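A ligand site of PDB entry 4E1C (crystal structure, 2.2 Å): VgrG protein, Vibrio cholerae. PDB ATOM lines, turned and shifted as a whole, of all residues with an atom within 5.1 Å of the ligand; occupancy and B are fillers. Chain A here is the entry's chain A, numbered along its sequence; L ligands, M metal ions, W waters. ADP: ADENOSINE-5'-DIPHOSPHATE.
O of Ser 93 is in hydrogen-bond range of O2' of the ligand (2.7 Å). The side-chain hydroxyl of Ser 24 sits at hydrogen-bond distance from a nitrogen (N1) of the ligand. An oxygen (O3') of the ligand lies within hydrogen-bond range of the backbone NH (N) of Ile 27 (3.1 Å). The backbone carbonyl oxygen (O) of Ile 27 is in hydrogen-bond range of an oxygen (O3') of the ligand (3.0 Å). The backbone NH of Gly 26 lies within hydrogen-bond range of a nitrogen (N3) of the ligand (3.4 Å). NH2 of Arg 280 is in salt-bridge range of O1B of the ligand (3.5 Å).
Water W7 bridges O1B of the ligand (2.7 Å) and NH2 of Arg 280 (3.4 Å). Water W2 lies within hydrogen-bond range of the side-chain carboxylate (OE1) of Glu 28 (2.6 Å), the side-chain hydroxyl (OG1) of Thr 176 (2.7 Å) and an oxygen (O3') of the ligand (2.9 Å). Water W6 bridges N7 of the ligand (2.9 Å) and O of Pro 17 (2.9 Å). Water W5 lies within hydrogen-bond range of a nitrogen (N6) of the ligand, the backbone carbonyl oxygen (O) of Thr 18 and the side-chain hydroxyl (OG) of Ser 24. Water W8 bridges OG1 of Thr 176 (2.7 Å) and NE of Arg 280 (3.0 Å).
N3 of the ligand lies close to O of Thr 176 (3.5 Å). Phe 16 touches the ligand. Ile 25 touches the ligand. CG of Glu 28 touches O3' of the ligand, 3.6 Å away. Val 92 touches the ligand. CG of Pro 95 touches C5 of the ligand, at 3.5 Å. Ile 333 touches the ligand. Ala 336 touches the ligand (CB to N6, 3.8 Å). Leu 349 touches the ligand. Hydrophobic or aromatic side chains within 4 Å of the ligand: Phe 16, Val 92, Pro 95, Ile 333, Ala 336 and Leu 349. The nearest printed residue that does not touch the ligand is Gly 178 (4.001 Å).
The backbone NH (N) of Ile 27 sits at hydrogen-bond distance from the side-chain hydroxyl (OG) of Ser 93 (2.8 Å). The backbone carbonyl oxygen (O) of Ser 24 lies within hydrogen-bond range of the backbone NH (N) of Gly 178 (2.8 Å). The backbone carbonyl oxygen (O) of Gly 26 lies within hydrogen-bond range of the backbone NH (N) of Thr 176 (2.8 Å). The backbone carbonyl oxygen of Leu 349 lies within hydrogen-bond range of the backbone NH of Arg 280 (2.7 Å). The backbone carbonyl oxygen (O) of Arg 280 is in hydrogen-bond range of the backbone NH (N) of Ile 333 (2.8 Å).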
ATOM      1  N   PHE A  16      19.765 -27.090   8.625  1.00  0.00           N
ATOM      2  CA  PHE A  16      19.162 -26.214   7.629  1.00  0.00           C
ATOM      3  C   PHE A  16      19.761 -26.500   6.252  1.00  0.00           C
ATOM      4  O   PHE A  16      20.973 -26.689   6.168  1.00  0.00           O
ATOM      5  CB  PHE A  16      19.453 -24.731   7.957  1.00  0.00           C
ATOM      6  CG  PHE A  16      18.880 -24.129   9.208  1.00  0.00           C
ATOM      7  CD1 PHE A  16      17.533 -24.309   9.533  1.00  0.00           C
ATOM      8  CD2 PHE A  16      19.655 -23.342  10.046  1.00  0.00           C
ATOM      9  CE1 PHE A  16      16.993 -23.709  10.671  1.00  0.00           C
ATOM     10  CE2 PHE A  16      19.111 -22.750  11.187  1.00  0.00           C
ATOM     11  CZ  PHE A  16      17.783 -22.939  11.491  1.00  0.00           C
ATOM     12  N   PRO A  17      18.968 -26.475   5.161  1.00  0.00           N
ATOM     13  CA  PRO A  17      19.597 -26.515   3.828  1.00  0.00           C
ATOM     14  C   PRO A  17      20.444 -25.225   3.686  1.00  0.00           C
ATOM     15  O   PRO A  17      20.075 -24.189   4.232  1.00  0.00           O
ATOM     16  CB  PRO A  17      18.405 -26.507   2.857  1.00  0.00           C
ATOM     17  CG  PRO A  17      17.262 -25.957   3.631  1.00  0.00           C
ATOM     18  CD  PRO A  17      17.509 -26.223   5.077  1.00  0.00           C
ATOM     19  N   THR A  18      21.593 -25.314   3.023  1.00  0.00           N
ATOM     20  CA  THR A  18      22.513 -24.186   2.851  1.00  0.00           C
ATOM     21  C   THR A  18      22.368 -23.451   1.520  1.00  0.00           C
ATOM     22  O   THR A  18      22.657 -22.258   1.478  1.00  0.00           O
ATOM     23  CB  THR A  18      23.958 -24.644   3.090  1.00  0.00           C
ATOM     24  OG1 THR A  18      24.272 -25.695   2.175  1.00  0.00           O
ATOM     25  CG2 THR A  18      24.219 -25.095   4.514  1.00  0.00           C
ATOM     26  N   PHE A  20      20.244 -22.071  -1.990  1.00  0.00           N
ATOM     27  CA  PHE A  20      18.993 -21.567  -2.560  1.00  0.00           C
ATOM     28  C   PHE A  20      19.333 -20.889  -3.903  1.00  0.00           C
ATOM     29  O   PHE A  20      20.382 -20.260  -4.002  1.00  0.00           O
ATOM     30  CB  PHE A  20      18.276 -20.592  -1.598  1.00  0.00           C
ATOM     31  CG  PHE A  20      17.706 -21.334  -0.403  1.00  0.00           C
ATOM     32  CD1 PHE A  20      16.507 -22.042  -0.512  1.00  0.00           C
ATOM     33  CD2 PHE A  20      18.424 -21.416   0.788  1.00  0.00           C
ATOM     34  CE1 PHE A  20      16.029 -22.806   0.548  1.00  0.00           C
ATOM     35  CE2 PHE A  20      17.946 -22.180   1.848  1.00  0.00           C
ATOM     36  CZ  PHE A  20      16.743 -22.854   1.725  1.00  0.00           C
ATOM     37  N   SER A  24      16.810 -15.934   0.102  1.00  0.00           N
ATOM     38  CA  SER A  24      16.131 -16.835   1.030  1.00  0.00           C
ATOM     39  C   SER A  24      15.658 -16.135   2.291  1.00  0.00           C
ATOM     40  O   SER A  24      16.122 -15.061   2.624  1.00  0.00           O
ATOM     41  CB  SER A  24      17.042 -18.011   1.353  1.00  0.00           C
ATOM     42  OG  SER A  24      18.315 -17.539   1.737  1.00  0.00           O
ATOM     43  N   ILE A  25      14.713 -16.768   2.980  1.00  0.00           N
ATOM     44  CA  ILE A  25      14.123 -16.243   4.211  1.00  0.00           C
ATOM     45  C   ILE A  25      13.864 -17.362   5.236  1.00  0.00           C
ATOM     46  O   ILE A  25      13.453 -18.448   4.868  1.00  0.00           O
ATOM     47  CB  ILE A  25      12.871 -15.362   3.930  1.00  0.00           C
ATOM     48  CG1 ILE A  25      12.375 -14.620   5.199  1.00  0.00           C
ATOM     49  CG2 ILE A  25      11.743 -16.145   3.208  1.00  0.00           C
ATOM     50  CD1 ILE A  25      11.702 -13.268   4.976  1.00  0.00           C
ATOM     51  N   GLY A  26      14.174 -17.052   6.485  1.00  0.00           N
ATOM     52  CA  GLY A  26      13.938 -17.904   7.635  1.00  0.00           C
ATOM     53  C   GLY A  26      13.235 -17.059   8.660  1.00  0.00           C
ATOM     54  O   GLY A  26      13.368 -15.833   8.647  1.00  0.00           O
ATOM     55  N   ILE A  27      12.446 -17.692   9.533  1.00  0.00           N
ATOM     56  CA  ILE A  27      11.717 -16.972  10.582  1.00  0.00           C
ATOM     57  C   ILE A  27      11.992 -17.612  11.953  1.00  0.00           C
ATOM     58  O   ILE A  27      12.369 -18.780  12.009  1.00  0.00           O
ATOM     59  CB  ILE A  27      10.203 -16.789  10.295  1.00  0.00           C
ATOM     60  CG1 ILE A  27       9.426 -18.135  10.210  1.00  0.00           C
ATOM     61  CG2 ILE A  27       9.961 -15.879   9.069  1.00  0.00           C
ATOM     62  CD1 ILE A  27       7.873 -18.041  10.305  1.00  0.00           C
ATOM     63  N   GLU A  28      11.835 -16.830  13.024  1.00  0.00           N
ATOM     64  CA  GLU A  28      11.972 -17.258  14.423  1.00  0.00           C
ATOM     65  C   GLU A  28      10.746 -16.745  15.127  1.00  0.00           C
ATOM     66  O   GLU A  28      10.366 -15.587  14.922  1.00  0.00           O
ATOM     67  CB  GLU A  28      13.230 -16.666  15.076  1.00  0.00           C
ATOM     68  CG  GLU A  28      14.525 -17.286  14.594  1.00  0.00           C
ATOM     69  CD  GLU A  28      15.748 -16.457  14.944  1.00  0.00           C
ATOM     70  OE1 GLU A  28      15.938 -15.367  14.357  1.00  0.00           O
ATOM     71  OE2 GLU A  28      16.519 -16.903  15.833  1.00  0.00           O
ATOM     72  N   GLN A  44      19.823 -27.366  22.030  1.00  0.00           N
ATOM     73  CA  GLN A  44      18.757 -26.402  21.732  1.00  0.00           C
ATOM     74  C   GLN A  44      17.527 -27.063  21.104  1.00  0.00           C
ATOM     75  O   GLN A  44      16.399 -26.775  21.505  1.00  0.00           O
ATOM     76  CB  GLN A  44      19.319 -25.322  20.789  1.00  0.00           C
ATOM     77  CG  GLN A  44      18.638 -23.967  20.916  1.00  0.00           C
ATOM     78  CD  GLN A  44      19.298 -23.066  21.940  1.00  0.00           C
ATOM     79  OE1 GLN A  44      19.914 -23.509  22.927  1.00  0.00           O
ATOM     80  NE2 GLN A  44      19.141 -21.755  21.726  1.00  0.00           N
ATOM     81  N   GLU A  90      10.938 -21.591  21.126  1.00  0.00           N
ATOM     82  CA  GLU A  90      11.027 -20.808  19.916  1.00  0.00           C
ATOM     83  C   GLU A  90      10.904 -21.724  18.700  1.00  0.00           C
ATOM     84  O   GLU A  90      11.639 -22.695  18.568  1.00  0.00           O
ATOM     85  CB  GLU A  90      12.315 -19.988  19.877  1.00  0.00           C
ATOM     86  CG  GLU A  90      12.327 -19.002  18.725  1.00  0.00           C
ATOM     87  CD  GLU A  90      13.616 -18.209  18.631  1.00  0.00           C
ATOM     88  OE1 GLU A  90      14.696 -18.828  18.749  1.00  0.00           O
ATOM     89  OE2 GLU A  90      13.539 -16.979  18.428  1.00  0.00           O
ATOM     90  N   VAL A  92      11.655 -22.274  14.959  1.00  0.00           N
ATOM     91  CA  VAL A  92      12.680 -21.804  14.022  1.00  0.00           C
ATOM     92  C   VAL A  92      12.483 -22.466  12.665  1.00  0.00           C
ATOM     93  O   VAL A  92      12.765 -23.652  12.524  1.00  0.00           O
ATOM     94  CB  VAL A  92      14.116 -22.017  14.606  1.00  0.00           C
ATOM     95  CG1 VAL A  92      15.177 -21.419  13.686  1.00  0.00           C
ATOM     96  CG2 VAL A  92      14.247 -21.424  16.024  1.00  0.00           C
ATOM     97  N   SER A  93      11.996 -21.710  11.671  1.00  0.00           N
ATOM     98  CA  SER A  93      11.778 -22.280  10.344  1.00  0.00           C
ATOM     99  C   SER A  93      13.051 -22.752   9.627  1.00  0.00           C
ATOM    100  O   SER A  93      14.148 -22.251   9.860  1.00  0.00           O
ATOM    101  CB  SER A  93      10.979 -21.348   9.451  1.00  0.00           C
ATOM    102  OG  SER A  93      11.808 -20.349   8.866  1.00  0.00           O
ATOM    103  N   TYR A  94      12.857 -23.703   8.732  1.00  0.00           N
ATOM    104  CA  TYR A  94      13.896 -24.132   7.822  1.00  0.00           C
ATOM    105  C   TYR A  94      13.791 -23.083   6.704  1.00  0.00           C
ATOM    106  O   TYR A  94      12.659 -22.744   6.328  1.00  0.00           O
ATOM    107  CB  TYR A  94      13.631 -25.557   7.313  1.00  0.00           C
ATOM    108  CG  TYR A  94      14.051 -26.594   8.327  1.00  0.00           C
ATOM    109  CD1 TYR A  94      13.200 -26.982   9.358  1.00  0.00           C
ATOM    110  CD2 TYR A  94      15.307 -27.196   8.259  1.00  0.00           C
ATOM    111  CE1 TYR A  94      13.583 -27.933  10.297  1.00  0.00           C
ATOM    112  CE2 TYR A  94      15.713 -28.145   9.204  1.00  0.00           C
ATOM    113  CZ  TYR A  94      14.845 -28.503  10.225  1.00  0.00           C
ATOM    114  OH  TYR A  94      15.233 -29.421  11.183  1.00  0.00           O
ATOM    115  N   PRO A  95      14.907 -22.476   6.243  1.00  0.00           N
ATOM    116  CA  PRO A  95      14.785 -21.423   5.212  1.00  0.00           C
ATOM    117  C   PRO A  95      14.140 -21.908   3.922  1.00  0.00           C
ATOM    118  O   PRO A  95      14.206 -23.085   3.567  1.00  0.00           O
ATOM    119  CB  PRO A  95      16.237 -20.978   4.980  1.00  0.00           C
ATOM    120  CG  PRO A  95      17.081 -22.150   5.431  1.00  0.00           C
ATOM    121  CD  PRO A  95      16.330 -22.708   6.597  1.00  0.00           C
ATOM    122  N   THR A 176      15.044 -13.653   9.007  1.00  0.00           N
ATOM    123  CA  THR A 176      16.429 -13.654   8.546  1.00  0.00           C
ATOM    124  C   THR A 176      16.409 -13.776   7.034  1.00  0.00           C
ATOM    125  O   THR A 176      15.811 -14.689   6.509  1.00  0.00           O
ATOM    126  CB  THR A 176      17.276 -14.740   9.245  1.00  0.00           C
ATOM    127  OG1 THR A 176      17.371 -14.439  10.649  1.00  0.00           O
ATOM    128  CG2 THR A 176      18.703 -14.826   8.693  1.00  0.00           C
ATOM    129  N   VAL A 177      17.088 -12.857   6.340  1.00  0.00           N
ATOM    130  CA  VAL A 177      17.101 -12.827   4.890  1.00  0.00           C
ATOM    131  C   VAL A 177      18.502 -13.129   4.433  1.00  0.00           C
ATOM    132  O   VAL A 177      19.455 -12.586   4.976  1.00  0.00           O
ATOM    133  CB  VAL A 177      16.532 -11.467   4.331  1.00  0.00           C
ATOM    134  CG1 VAL A 177      16.759 -11.331   2.817  1.00  0.00           C
ATOM    135  CG2 VAL A 177      15.043 -11.300   4.671  1.00  0.00           C
ATOM    136  N   GLY A 178      18.610 -13.989   3.424  1.00  0.00           N
ATOM    137  CA  GLY A 178      19.876 -14.372   2.823  1.00  0.00           C
ATOM    138  C   GLY A 178      19.924 -13.926   1.379  1.00  0.00           C
ATOM    139  O   GLY A 178      18.971 -14.191   0.654  1.00  0.00           O
ATOM    140  N   ARG A 280      24.507 -11.553   9.991  1.00  0.00           N
ATOM    141  CA  ARG A 280      24.578 -12.874  10.583  1.00  0.00           C
ATOM    142  C   ARG A 280      25.710 -13.717  10.022  1.00  0.00           C
ATOM    143  O   ARG A 280      25.922 -14.823  10.503  1.00  0.00           O
ATOM    144  CB  ARG A 280      23.221 -13.604  10.419  1.00  0.00           C
ATOM    145  CG  ARG A 280      22.093 -12.991  11.285  1.00  0.00           C
ATOM    146  CD  ARG A 280      22.270 -13.251  12.783  1.00  0.00           C
ATOM    147  NE  ARG A 280      22.208 -14.693  13.084  1.00  0.00           N
ATOM    148  CZ  ARG A 280      23.242 -15.405  13.511  1.00  0.00           C
ATOM    149  NH1 ARG A 280      24.413 -14.828  13.756  1.00  0.00           N
ATOM    150  NH2 ARG A 280      23.103 -16.708  13.743  1.00  0.00           N
ATOM    151  N   ILE A 333      26.081 -17.596  10.328  1.00  0.00           N
ATOM    152  CA  ILE A 333      25.630 -18.536   9.301  1.00  0.00           C
ATOM    153  C   ILE A 333      26.596 -18.254   8.123  1.00  0.00           C
ATOM    154  O   ILE A 333      26.401 -17.309   7.346  1.00  0.00           O
ATOM    155  CB  ILE A 333      24.111 -18.372   8.946  1.00  0.00           C
ATOM    156  CG1 ILE A 333      23.238 -18.573  10.219  1.00  0.00           C
ATOM    157  CG2 ILE A 333      23.704 -19.388   7.846  1.00  0.00           C
ATOM    158  CD1 ILE A 333      21.859 -17.898  10.208  1.00  0.00           C
ATOM    159  N   ALA A 336      26.165 -20.644   3.950  1.00  0.00           N
ATOM    160  CA  ALA A 336      24.995 -20.455   3.085  1.00  0.00           C
ATOM    161  C   ALA A 336      25.473 -19.989   1.713  1.00  0.00           C
ATOM    162  O   ALA A 336      26.466 -19.257   1.600  1.00  0.00           O
ATOM    163  CB  ALA A 336      24.030 -19.450   3.686  1.00  0.00           C
ATOM    164  N   LEU A 349      23.772 -13.254   5.307  1.00  0.00           N
ATOM    165  CA  LEU A 349      22.492 -13.212   5.999  1.00  0.00           C
ATOM    166  C   LEU A 349      22.333 -12.060   6.969  1.00  0.00           C
ATOM    167  O   LEU A 349      23.299 -11.552   7.535  1.00  0.00           O
ATOM    168  CB  LEU A 349      22.285 -14.556   6.717  1.00  0.00           C
ATOM    169  CG  LEU A 349      21.633 -15.678   5.895  1.00  0.00           C
ATOM    170  CD1 LEU A 349      22.557 -16.201   4.789  1.00  0.00           C
ATOM    171  CD2 LEU A 349      21.299 -16.812   6.773  1.00  0.00           C
HETATM  172  PB  ADP L   1      20.290 -19.161  16.597  1.00  0.00           P
HETATM  173  O1B ADP L   1      21.618 -18.631  16.237  1.00  0.00           O
HETATM  174  O2B ADP L   1      20.452 -20.493  17.378  1.00  0.00           O
HETATM  175  O3B ADP L   1      19.545 -18.147  17.480  1.00  0.00           O
HETATM  176  PA  ADP L   1      19.851 -20.132  13.873  1.00  0.00           P
HETATM  177  O1A ADP L   1      21.320 -19.968  13.636  1.00  0.00           O
HETATM  178  O2A ADP L   1      19.506 -21.620  13.971  1.00  0.00           O
HETATM  179  O3A ADP L   1      19.451 -19.424  15.263  1.00  0.00           O
HETATM  180  O5' ADP L   1      19.061 -19.459  12.683  1.00  0.00           O
HETATM  181  C5' ADP L   1      18.305 -18.257  12.819  1.00  0.00           C
HETATM  182  C4' ADP L   1      17.513 -18.012  11.559  1.00  0.00           C
HETATM  183  O4' ADP L   1      18.345 -18.154  10.393  1.00  0.00           O
HETATM  184  C3' ADP L   1      16.272 -18.895  11.333  1.00  0.00           C
HETATM  185  O3' ADP L   1      15.157 -18.051  11.092  1.00  0.00           O
HETATM  186  C2' ADP L   1      16.638 -19.684  10.070  1.00  0.00           C
HETATM  187  O2' ADP L   1      15.571 -20.089   9.234  1.00  0.00           O
HETATM  188  C1' ADP L   1      17.508 -18.650   9.377  1.00  0.00           C
HETATM  189  N9  ADP L   1      18.311 -19.163   8.273  1.00  0.00           N
HETATM  190  C8  ADP L   1      19.225 -20.180   8.288  1.00  0.00           C
HETATM  191  N7  ADP L   1      19.781 -20.404   7.131  1.00  0.00           N
HETATM  192  C5  ADP L   1      19.209 -19.467   6.291  1.00  0.00           C
HETATM  193  C6  ADP L   1      19.404 -19.158   4.927  1.00  0.00           C
HETATM  194  N6  ADP L   1      20.270 -19.816   4.139  1.00  0.00           N
HETATM  195  N1  ADP L   1      18.683 -18.147   4.406  1.00  0.00           N
HETATM  196  C2  ADP L   1      17.815 -17.493   5.185  1.00  0.00           C
HETATM  197  N3  ADP L   1      17.540 -17.692   6.469  1.00  0.00           N
HETATM  198  C4  ADP L   1      18.287 -18.701   6.975  1.00  0.00           C
HETATM  199 MG    MG M   1      17.137 -18.991  16.945  1.00  0.00          MG
HETATM  200  O   HOH W   1      18.735 -15.020  18.376  1.00  0.00           O
HETATM  201  O   HOH W   2      15.165 -15.292  11.863  1.00  0.00           O
HETATM  202  O   HOH W   3      20.755 -24.643  13.297  1.00  0.00           O
HETATM  203  O   HOH W   4      18.214 -23.128  16.383  1.00  0.00           O
HETATM  204  O   HOH W   5      21.254 -19.226   1.262  1.00  0.00           O
HETATM  205  O   HOH W   6      21.555 -22.272   5.870  1.00  0.00           O
HETATM  206  O   HOH W   7      22.053 -16.067  16.930  1.00  0.00           O
HETATM  207  O   HOH W   8      19.318 -15.055  12.349  1.00  0.00           O
HETATM  208  O   HOH W   9      20.672 -23.859  17.938  1.00  0.00           O
HETATM  209  O   HOH W  10      19.216 -16.027  15.546  1.00  0.00           O
